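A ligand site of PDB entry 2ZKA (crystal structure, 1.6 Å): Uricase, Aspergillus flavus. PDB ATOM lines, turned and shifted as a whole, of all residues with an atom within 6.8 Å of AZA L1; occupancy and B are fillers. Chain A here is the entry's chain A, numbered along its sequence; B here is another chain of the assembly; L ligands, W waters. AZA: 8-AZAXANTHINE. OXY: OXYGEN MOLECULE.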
ATOM      1  N   SER A 158     -22.020  -5.916  11.871  1.00  0.00           N
ATOM      2  CA  SER A 158     -21.773  -6.094  13.293  1.00  0.00           C
ATOM      3  C   SER A 158     -20.858  -4.947  13.719  1.00  0.00           C
ATOM      4  O   SER A 158     -19.915  -4.592  13.013  1.00  0.00           O
ATOM      5  CB  SER A 158     -21.087  -7.450  13.557  1.00  0.00           C
ATOM      6  OG  SER A 158     -20.582  -7.538  14.889  1.00  0.00           O
ATOM      7  N   GLN A 159     -21.162  -4.364  14.870  1.00  0.00           N
ATOM      8  CA  GLN A 159     -20.428  -3.240  15.405  1.00  0.00           C
ATOM      9  C   GLN A 159     -20.103  -3.525  16.853  1.00  0.00           C
ATOM     10  O   GLN A 159     -20.762  -4.357  17.514  1.00  0.00           O
ATOM     11  CB  GLN A 159     -21.291  -1.946  15.336  1.00  0.00           C
ATOM     12  CG  GLN A 159     -21.819  -1.655  13.940  1.00  0.00           C
ATOM     13  CD  GLN A 159     -22.612  -0.359  13.858  1.00  0.00           C
ATOM     14  OE1 GLN A 159     -22.700   0.411  14.819  1.00  0.00           O
ATOM     15  NE2 GLN A 159     -23.202  -0.122  12.704  1.00  0.00           N
ATOM     16  N   PHE A 160     -19.118  -2.816  17.371  1.00  0.00           N
ATOM     17  CA  PHE A 160     -18.856  -2.837  18.792  1.00  0.00           C
ATOM     18  C   PHE A 160     -18.093  -1.592  19.220  1.00  0.00           C
ATOM     19  O   PHE A 160     -16.885  -1.492  19.056  1.00  0.00           O
ATOM     20  CB  PHE A 160     -18.152  -4.142  19.237  1.00  0.00           C
ATOM     21  CG  PHE A 160     -18.151  -4.328  20.737  1.00  0.00           C
ATOM     22  CD1 PHE A 160     -19.357  -4.451  21.434  1.00  0.00           C
ATOM     23  CD2 PHE A 160     -16.956  -4.303  21.466  1.00  0.00           C
ATOM     24  CE1 PHE A 160     -19.374  -4.573  22.811  1.00  0.00           C
ATOM     25  CE2 PHE A 160     -16.961  -4.452  22.851  1.00  0.00           C
ATOM     26  CZ  PHE A 160     -18.183  -4.558  23.541  1.00  0.00           C
ATOM     27  N   PHE A 163     -18.007   0.845  24.603  1.00  0.00           N
ATOM     28  CA  PHE A 163     -17.712   0.096  25.833  1.00  0.00           C
ATOM     29  C   PHE A 163     -16.789   0.846  26.795  1.00  0.00           C
ATOM     30  O   PHE A 163     -16.156   1.841  26.406  1.00  0.00           O
ATOM     31  CB  PHE A 163     -17.089  -1.279  25.507  1.00  0.00           C
ATOM     32  CG  PHE A 163     -15.969  -1.207  24.535  1.00  0.00           C
ATOM     33  CD1 PHE A 163     -16.216  -1.231  23.172  1.00  0.00           C
ATOM     34  CD2 PHE A 163     -14.647  -1.095  24.994  1.00  0.00           C
ATOM     35  CE1 PHE A 163     -15.169  -1.156  22.249  1.00  0.00           C
ATOM     36  CE2 PHE A 163     -13.603  -1.028  24.086  1.00  0.00           C
ATOM     37  CZ  PHE A 163     -13.864  -1.035  22.730  1.00  0.00           C
ATOM     38  N   LEU A 171      -8.569  -2.421  23.139  1.00  0.00           N
ATOM     39  CA  LEU A 171      -9.457  -2.696  22.018  1.00  0.00           C
ATOM     40  C   LEU A 171      -9.948  -1.401  21.371  1.00  0.00           C
ATOM     41  O   LEU A 171     -10.432  -0.492  22.082  1.00  0.00           O
ATOM     42  CB  LEU A 171     -10.677  -3.495  22.519  1.00  0.00           C
ATOM     43  CG  LEU A 171     -11.694  -3.929  21.445  1.00  0.00           C
ATOM     44  CD1 LEU A 171     -11.059  -4.935  20.490  1.00  0.00           C
ATOM     45  CD2 LEU A 171     -12.901  -4.546  22.107  1.00  0.00           C
ATOM     46  N   ARG A 177     -17.373  -5.125  11.713  1.00  0.00           N
ATOM     47  CA  ARG A 177     -16.510  -6.292  12.011  1.00  0.00           C
ATOM     48  C   ARG A 177     -17.210  -7.565  11.565  1.00  0.00           C
ATOM     49  O   ARG A 177     -18.387  -7.575  11.246  1.00  0.00           O
ATOM     50  CB  ARG A 177     -16.174  -6.349  13.505  1.00  0.00           C
ATOM     51  CG  ARG A 177     -17.384  -6.644  14.352  1.00  0.00           C
ATOM     52  CD  ARG A 177     -17.049  -6.715  15.812  1.00  0.00           C
ATOM     53  NE  ARG A 177     -18.245  -7.144  16.564  1.00  0.00           N
ATOM     54  CZ  ARG A 177     -18.270  -7.466  17.859  1.00  0.00           C
ATOM     55  NH1 ARG A 177     -17.167  -7.389  18.614  1.00  0.00           N
ATOM     56  NH2 ARG A 177     -19.422  -7.853  18.413  1.00  0.00           N
ATOM     57  N   LEU A 179     -18.716 -11.190  12.597  1.00  0.00           N
ATOM     58  CA  LEU A 179     -19.273 -11.849  13.774  1.00  0.00           C
ATOM     59  C   LEU A 179     -19.532 -13.314  13.448  1.00  0.00           C
ATOM     60  O   LEU A 179     -20.240 -13.643  12.493  1.00  0.00           O
ATOM     61  CB  LEU A 179     -20.566 -11.158  14.223  1.00  0.00           C
ATOM     62  CG  LEU A 179     -21.266 -11.741  15.444  1.00  0.00           C
ATOM     63  CD1 LEU A 179     -20.329 -11.742  16.650  1.00  0.00           C
ATOM     64  CD2 LEU A 179     -22.566 -10.959  15.754  1.00  0.00           C
ATOM     65  N   SER A 225     -25.944  -5.577  14.362  1.00  0.00           N
ATOM     66  CA  SER A 225     -25.685  -5.950  15.727  1.00  0.00           C
ATOM     67  C   SER A 225     -24.834  -4.945  16.485  1.00  0.00           C
ATOM     68  O   SER A 225     -23.740  -4.588  16.057  1.00  0.00           O
ATOM     69  CB  SER A 225     -24.999  -7.316  15.715  1.00  0.00           C
ATOM     70  OG  SER A 225     -24.600  -7.645  17.024  1.00  0.00           O
ATOM     71  N   ALA A 226     -25.320  -4.513  17.636  1.00  0.00           N
ATOM     72  CA  ALA A 226     -24.618  -3.579  18.480  1.00  0.00           C
ATOM     73  C   ALA A 226     -23.626  -4.294  19.387  1.00  0.00           C
ATOM     74  O   ALA A 226     -22.724  -3.676  19.958  1.00  0.00           O
ATOM     75  CB  ALA A 226     -25.638  -2.787  19.342  1.00  0.00           C
ATOM     76  N   SER A 227     -23.828  -5.614  19.540  1.00  0.00           N
ATOM     77  CA  SER A 227     -23.001  -6.469  20.403  1.00  0.00           C
ATOM     78  C   SER A 227     -23.620  -7.844  20.345  1.00  0.00           C
ATOM     79  O   SER A 227     -24.771  -7.993  19.930  1.00  0.00           O
ATOM     80  CB  SER A 227     -22.960  -6.009  21.863  1.00  0.00           C
ATOM     81  OG  SER A 227     -24.277  -6.104  22.448  1.00  0.00           O
ATOM     82  N   VAL A 228     -22.891  -8.864  20.797  1.00  0.00           N
ATOM     83  CA  VAL A 228     -23.466 -10.194  20.875  1.00  0.00           C
ATOM     84  C   VAL A 228     -24.629 -10.158  21.874  1.00  0.00           C
ATOM     85  O   VAL A 228     -25.677 -10.752  21.633  1.00  0.00           O
ATOM     86  CB  VAL A 228     -22.376 -11.217  21.318  1.00  0.00           C
ATOM     87  CG1 VAL A 228     -22.974 -12.569  21.534  1.00  0.00           C
ATOM     88  CG2 VAL A 228     -21.298 -11.290  20.214  1.00  0.00           C
ATOM     89  N   GLN A 229     -24.411  -9.453  22.982  1.00  0.00           N
ATOM     90  CA  GLN A 229     -25.410  -9.298  24.047  1.00  0.00           C
ATOM     91  C   GLN A 229     -26.748  -8.823  23.465  1.00  0.00           C
ATOM     92  O   GLN A 229     -27.820  -9.409  23.738  1.00  0.00           O
ATOM     93  CB  GLN A 229     -24.932  -8.265  25.063  1.00  0.00           C
ATOM     94  CG  GLN A 229     -23.811  -8.760  26.005  1.00  0.00           C
ATOM     95  CD  GLN A 229     -22.391  -8.595  25.473  1.00  0.00           C
ATOM     96  OE1 GLN A 229     -22.147  -8.546  24.264  1.00  0.00           O
ATOM     97  NE2 GLN A 229     -21.422  -8.554  26.419  1.00  0.00           N
ATOM     98  N   ASN A 255     -17.724 -15.691  21.014  1.00  0.00           N
ATOM     99  CA  ASN A 255     -17.423 -14.724  19.988  1.00  0.00           C
ATOM    100  C   ASN A 255     -16.092 -15.194  19.370  1.00  0.00           C
ATOM    101  O   ASN A 255     -15.051 -15.099  20.017  1.00  0.00           O
ATOM    102  CB  ASN A 255     -17.346 -13.330  20.630  1.00  0.00           C
ATOM    103  CG  ASN A 255     -17.265 -12.213  19.608  1.00  0.00           C
ATOM    104  OD1 ASN A 255     -17.295 -12.438  18.406  1.00  0.00           O
ATOM    105  ND2 ASN A 255     -17.120 -10.980  20.103  1.00  0.00           N
ATOM    106  N   HIS A 257     -13.242 -14.850  17.182  1.00  0.00           N
ATOM    107  CA  HIS A 257     -12.660 -13.641  16.597  1.00  0.00           C
ATOM    108  C   HIS A 257     -11.927 -13.875  15.302  1.00  0.00           C
ATOM    109  O   HIS A 257     -11.211 -14.864  15.128  1.00  0.00           O
ATOM    110  CB  HIS A 257     -11.701 -12.991  17.602  1.00  0.00           C
ATOM    111  CG  HIS A 257     -12.302 -12.766  18.950  1.00  0.00           C
ATOM    112  ND1 HIS A 257     -13.362 -11.911  19.151  1.00  0.00           N
ATOM    113  CD2 HIS A 257     -12.021 -13.314  20.165  1.00  0.00           C
ATOM    114  CE1 HIS A 257     -13.686 -11.909  20.436  1.00  0.00           C
ATOM    115  NE2 HIS A 257     -12.887 -12.759  21.073  1.00  0.00           N
ATOM    116  N   GLY A 287     -14.390 -14.709  23.254  1.00  0.00           N
ATOM    117  CA  GLY A 287     -15.415 -14.183  24.170  1.00  0.00           C
ATOM    118  C   GLY A 287     -16.446 -15.271  24.404  1.00  0.00           C
ATOM    119  O   GLY A 287     -16.634 -16.183  23.593  1.00  0.00           O
ATOM    120  N   ILE A 289     -20.443 -15.272  25.921  1.00  0.00           N
ATOM    121  CA  ILE A 289     -21.543 -14.403  26.352  1.00  0.00           C
ATOM    122  C   ILE A 289     -22.768 -15.251  26.628  1.00  0.00           C
ATOM    123  O   ILE A 289     -23.143 -16.075  25.780  1.00  0.00           O
ATOM    124  CB  ILE A 289     -21.893 -13.358  25.249  1.00  0.00           C
ATOM    125  CG1 ILE A 289     -20.630 -12.755  24.583  1.00  0.00           C
ATOM    126  CG2 ILE A 289     -22.774 -12.263  25.865  1.00  0.00           C
ATOM    127  CD1 ILE A 289     -19.674 -12.092  25.461  1.00  0.00           C
ATOM    128  N   TYR B   9     -20.746 -12.909  31.284  1.00  0.00           N
ATOM    129  CA  TYR B   9     -20.009 -12.837  30.025  1.00  0.00           C
ATOM    130  C   TYR B   9     -18.518 -12.664  30.389  1.00  0.00           C
ATOM    131  O   TYR B   9     -18.170 -12.224  31.484  1.00  0.00           O
ATOM    132  CB  TYR B   9     -20.498 -11.682  29.142  1.00  0.00           C
ATOM    133  CG  TYR B   9     -19.882 -10.385  29.566  1.00  0.00           C
ATOM    134  CD1 TYR B   9     -20.251  -9.780  30.764  1.00  0.00           C
ATOM    135  CD2 TYR B   9     -18.849  -9.819  28.829  1.00  0.00           C
ATOM    136  CE1 TYR B   9     -19.602  -8.606  31.197  1.00  0.00           C
ATOM    137  CE2 TYR B   9     -18.220  -8.670  29.244  1.00  0.00           C
ATOM    138  CZ  TYR B   9     -18.600  -8.072  30.436  1.00  0.00           C
ATOM    139  OH  TYR B   9     -17.958  -6.929  30.850  1.00  0.00           O
ATOM    140  N   GLY B  10     -17.646 -13.005  29.463  1.00  0.00           N
ATOM    141  CA  GLY B  10     -16.211 -12.817  29.710  1.00  0.00           C
ATOM    142  C   GLY B  10     -15.372 -13.461  28.631  1.00  0.00           C
ATOM    143  O   GLY B  10     -15.770 -13.525  27.474  1.00  0.00           O
ATOM    144  N   LYS B  11     -14.198 -13.947  29.021  1.00  0.00           N
ATOM    145  CA  LYS B  11     -13.234 -14.495  28.040  1.00  0.00           C
ATOM    146  C   LYS B  11     -12.923 -15.917  28.453  1.00  0.00           C
ATOM    147  O   LYS B  11     -12.628 -16.179  29.626  1.00  0.00           O
ATOM    148  CB  LYS B  11     -11.935 -13.692  28.016  1.00  0.00           C
ATOM    149  CG  LYS B  11     -11.135 -13.858  26.706  1.00  0.00           C
ATOM    150  CD  LYS B  11     -11.900 -13.253  25.515  1.00  0.00           C
ATOM    151  CE  LYS B  11     -11.042 -12.441  24.590  1.00  0.00           C
ATOM    152  NZ  LYS B  11     -11.909 -11.664  23.635  1.00  0.00           N
ATOM    153  N   ASN B  52     -23.573  -0.249  25.719  1.00  0.00           N
ATOM    154  CA  ASN B  52     -22.252  -0.866  25.932  1.00  0.00           C
ATOM    155  C   ASN B  52     -21.428  -0.226  27.049  1.00  0.00           C
ATOM    156  O   ASN B  52     -20.349  -0.728  27.399  1.00  0.00           O
ATOM    157  CB  ASN B  52     -21.467  -0.961  24.620  1.00  0.00           C
ATOM    158  CG  ASN B  52     -22.091  -1.961  23.637  1.00  0.00           C
ATOM    159  OD1 ASN B  52     -22.780  -2.896  24.063  1.00  0.00           O
ATOM    160  ND2 ASN B  52     -21.854  -1.773  22.351  1.00  0.00           N
ATOM    161  N   ILE B  55     -20.168  -2.439  29.760  1.00  0.00           N
ATOM    162  CA  ILE B  55     -19.339  -3.602  29.386  1.00  0.00           C
ATOM    163  C   ILE B  55     -17.844  -3.350  29.533  1.00  0.00           C
ATOM    164  O   ILE B  55     -17.278  -2.480  28.850  1.00  0.00           O
ATOM    165  CB  ILE B  55     -19.595  -4.077  27.937  1.00  0.00           C
ATOM    166  CG1 ILE B  55     -21.040  -4.541  27.731  1.00  0.00           C
ATOM    167  CG2 ILE B  55     -18.606  -5.264  27.578  1.00  0.00           C
ATOM    168  CD1 ILE B  55     -21.375  -4.822  26.245  1.00  0.00           C
ATOM    169  N   VAL B  56     -17.230  -4.098  30.437  1.00  0.00           N
ATOM    170  CA  VAL B  56     -15.781  -4.251  30.463  1.00  0.00           C
ATOM    171  C   VAL B  56     -15.498  -5.219  29.310  1.00  0.00           C
ATOM    172  O   VAL B  56     -15.946  -6.364  29.369  1.00  0.00           O
ATOM    173  CB  VAL B  56     -15.314  -4.822  31.834  1.00  0.00           C
ATOM    174  CG1 VAL B  56     -13.808  -5.123  31.819  1.00  0.00           C
ATOM    175  CG2 VAL B  56     -15.679  -3.843  32.958  1.00  0.00           C
ATOM    176  N   ALA B  57     -14.810  -4.759  28.251  1.00  0.00           N
ATOM    177  CA  ALA B  57     -14.676  -5.581  27.040  1.00  0.00           C
ATOM    178  C   ALA B  57     -13.975  -6.894  27.365  1.00  0.00           C
ATOM    179  O   ALA B  57     -13.077  -6.929  28.207  1.00  0.00           O
ATOM    180  CB  ALA B  57     -13.928  -4.814  25.913  1.00  0.00           C
ATOM    181  N   THR B  58     -14.374  -7.976  26.700  1.00  0.00           N
ATOM    182  CA  THR B  58     -13.748  -9.259  26.995  1.00  0.00           C
ATOM    183  C   THR B  58     -12.263  -9.185  26.632  1.00  0.00           C
ATOM    184  O   THR B  58     -11.445  -9.822  27.315  1.00  0.00           O
ATOM    185  CB  THR B  58     -14.430 -10.432  26.266  1.00  0.00           C
ATOM    186  OG1 THR B  58     -14.221 -10.307  24.865  1.00  0.00           O
ATOM    187  CG2 THR B  58     -15.936 -10.424  26.592  1.00  0.00           C
ATOM    188  N   ASP B  59     -11.906  -8.406  25.608  1.00  0.00           N
ATOM    189  CA  ASP B  59     -10.482  -8.181  25.308  1.00  0.00           C
ATOM    190  C   ASP B  59      -9.710  -7.599  26.502  1.00  0.00           C
ATOM    191  O   ASP B  59      -8.576  -7.979  26.764  1.00  0.00           O
ATOM    192  CB  ASP B  59     -10.339  -7.247  24.104  1.00  0.00           C
ATOM    193  CG  ASP B  59      -8.923  -7.200  23.591  1.00  0.00           C
ATOM    194  OD1 ASP B  59      -8.507  -8.165  22.917  1.00  0.00           O
ATOM    195  OD2 ASP B  59      -8.239  -6.185  23.851  1.00  0.00           O
ATOM    196  N   SER B  60     -10.342  -6.658  27.218  1.00  0.00           N
ATOM    197  CA  SER B  60      -9.752  -6.092  28.450  1.00  0.00           C
ATOM    198  C   SER B  60      -9.625  -7.105  29.578  1.00  0.00           C
ATOM    199  O   SER B  60      -8.668  -7.083  30.362  1.00  0.00           O
ATOM    200  CB  SER B  60     -10.569  -4.863  28.913  1.00  0.00           C
ATOM    201  OG  SER B  60     -10.749  -3.977  27.824  1.00  0.00           O
HETATM  202  N1  AZA L   1     -19.386  -8.199  23.277  1.00  0.00           N
HETATM  203  C2  AZA L   1     -19.081  -8.152  21.956  1.00  0.00           C
HETATM  204  O2  AZA L   1     -20.001  -8.313  21.139  1.00  0.00           O
HETATM  205  N3  AZA L   1     -17.810  -7.964  21.471  1.00  0.00           N
HETATM  206  C4  AZA L   1     -16.824  -7.770  22.381  1.00  0.00           C
HETATM  207  C5  AZA L   1     -17.073  -7.790  23.788  1.00  0.00           C
HETATM  208  C6  AZA L   1     -18.455  -8.032  24.235  1.00  0.00           C
HETATM  209  O6  AZA L   1     -18.715  -8.084  25.445  1.00  0.00           O
HETATM  210  N7  AZA L   1     -15.892  -7.578  24.467  1.00  0.00           N
HETATM  211  N8  AZA L   1     -14.951  -7.444  23.437  1.00  0.00           N
HETATM  212  N9  AZA L   1     -15.486  -7.536  22.130  1.00  0.00           N
HETATM  213  O1  OXY L   2     -16.551 -11.105  23.498  1.00  0.00           O
HETATM  214  O2  OXY L   2     -15.897 -11.173  22.487  1.00  0.00           O
HETATM  215  O   HOH W   1     -14.070  -7.848  19.864  1.00  0.00           O
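Merely in contact with AZA L1: Phe 160 (3.4 Å), Ala 57 of chain B (3.5 Å), Ile 55 of chain B (3.5 Å), Ser 227 (3.6 Å), Leu 171 (3.8 Å), Tyr 9 of chain B (3.8 Å) and Asp 59 of chain B (3.9 Å).
Hydrophobic or aromatic side chains that line AZA L1: Phe 160, Leu 171, Val 228, Tyr 9 of chain B, Ile 55 of chain B and Ala 57 of chain B.
Of the 26 residues printed, 12 come within 4 Å of AZA L1.
The nearest printed residue that does not touch AZA L1 is Ile 289 (4.1 Å).
Water W1 bridges N9 of AZA L1 (2.7 Å) and NH1 of Arg 177 (3.4 Å).
The side-chain amide nitrogen of Asn 255 sits close to a nitrogen (N3) of AZA L1 (3.4 Å).
The side-chain amide nitrogen (NE2) of Gln 229 sits at hydrogen-bond distance from an oxygen (O6) of AZA L1 (2.9 Å).
The side-chain hydroxyl (OG1) of Thr 58 of chain B is in hydrogen-bond range of a nitrogen (N7) of AZA L1.
The guanidinium group of Arg 177 sits at hydrogen-bond distance from an oxygen (O2) of AZA L1 (2.8 Å).
An oxygen (O2) of AZA L1 is in hydrogen-bond range of the backbone NH (N) of Val 228, 3.0 Å away.
N of Thr 58 of chain B sits at hydrogen-bond distance from N7 of AZA L1, 2.7 Å away.
The side-chain amide nitrogen (ND2) of Asn 255 sits at hydrogen-bond distance from an oxygen (O2) of OXY L2 (2.7 Å).
O1 of OXY L2 lies within hydrogen-bond range of OG1 of Thr 58 of chain B (2.8 Å).
The side-chain hydroxyl of Ser 158 is in hydrogen-bond range of the guanidinium group of Arg 177, 2.9 Å away.
NE2 of His 257 is in hydrogen-bond range of O of Asn 255 (3.4 Å).
The side-chain hydroxyl (OH) of Tyr 9 of chain B lies within hydrogen-bond range of the backbone carbonyl oxygen (O) of Val 56 of chain B (2.6 Å).
OG of Ser 225 is in hydrogen-bond range of O of Ser 227 (2.9 Å).
The backbone NH (N) of Asn 255 sits at hydrogen-bond distance from the backbone carbonyl oxygen (O) of Gly 287, at 2.8 Å.
The side-chain hydroxyl of Thr 58 of chain B is in hydrogen-bond range of the side-chain amino group of Lys 11 of chain B, at 2.9 Å.
N of Gln 229 lies close to OG of Ser 227, at 3.4 Å.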
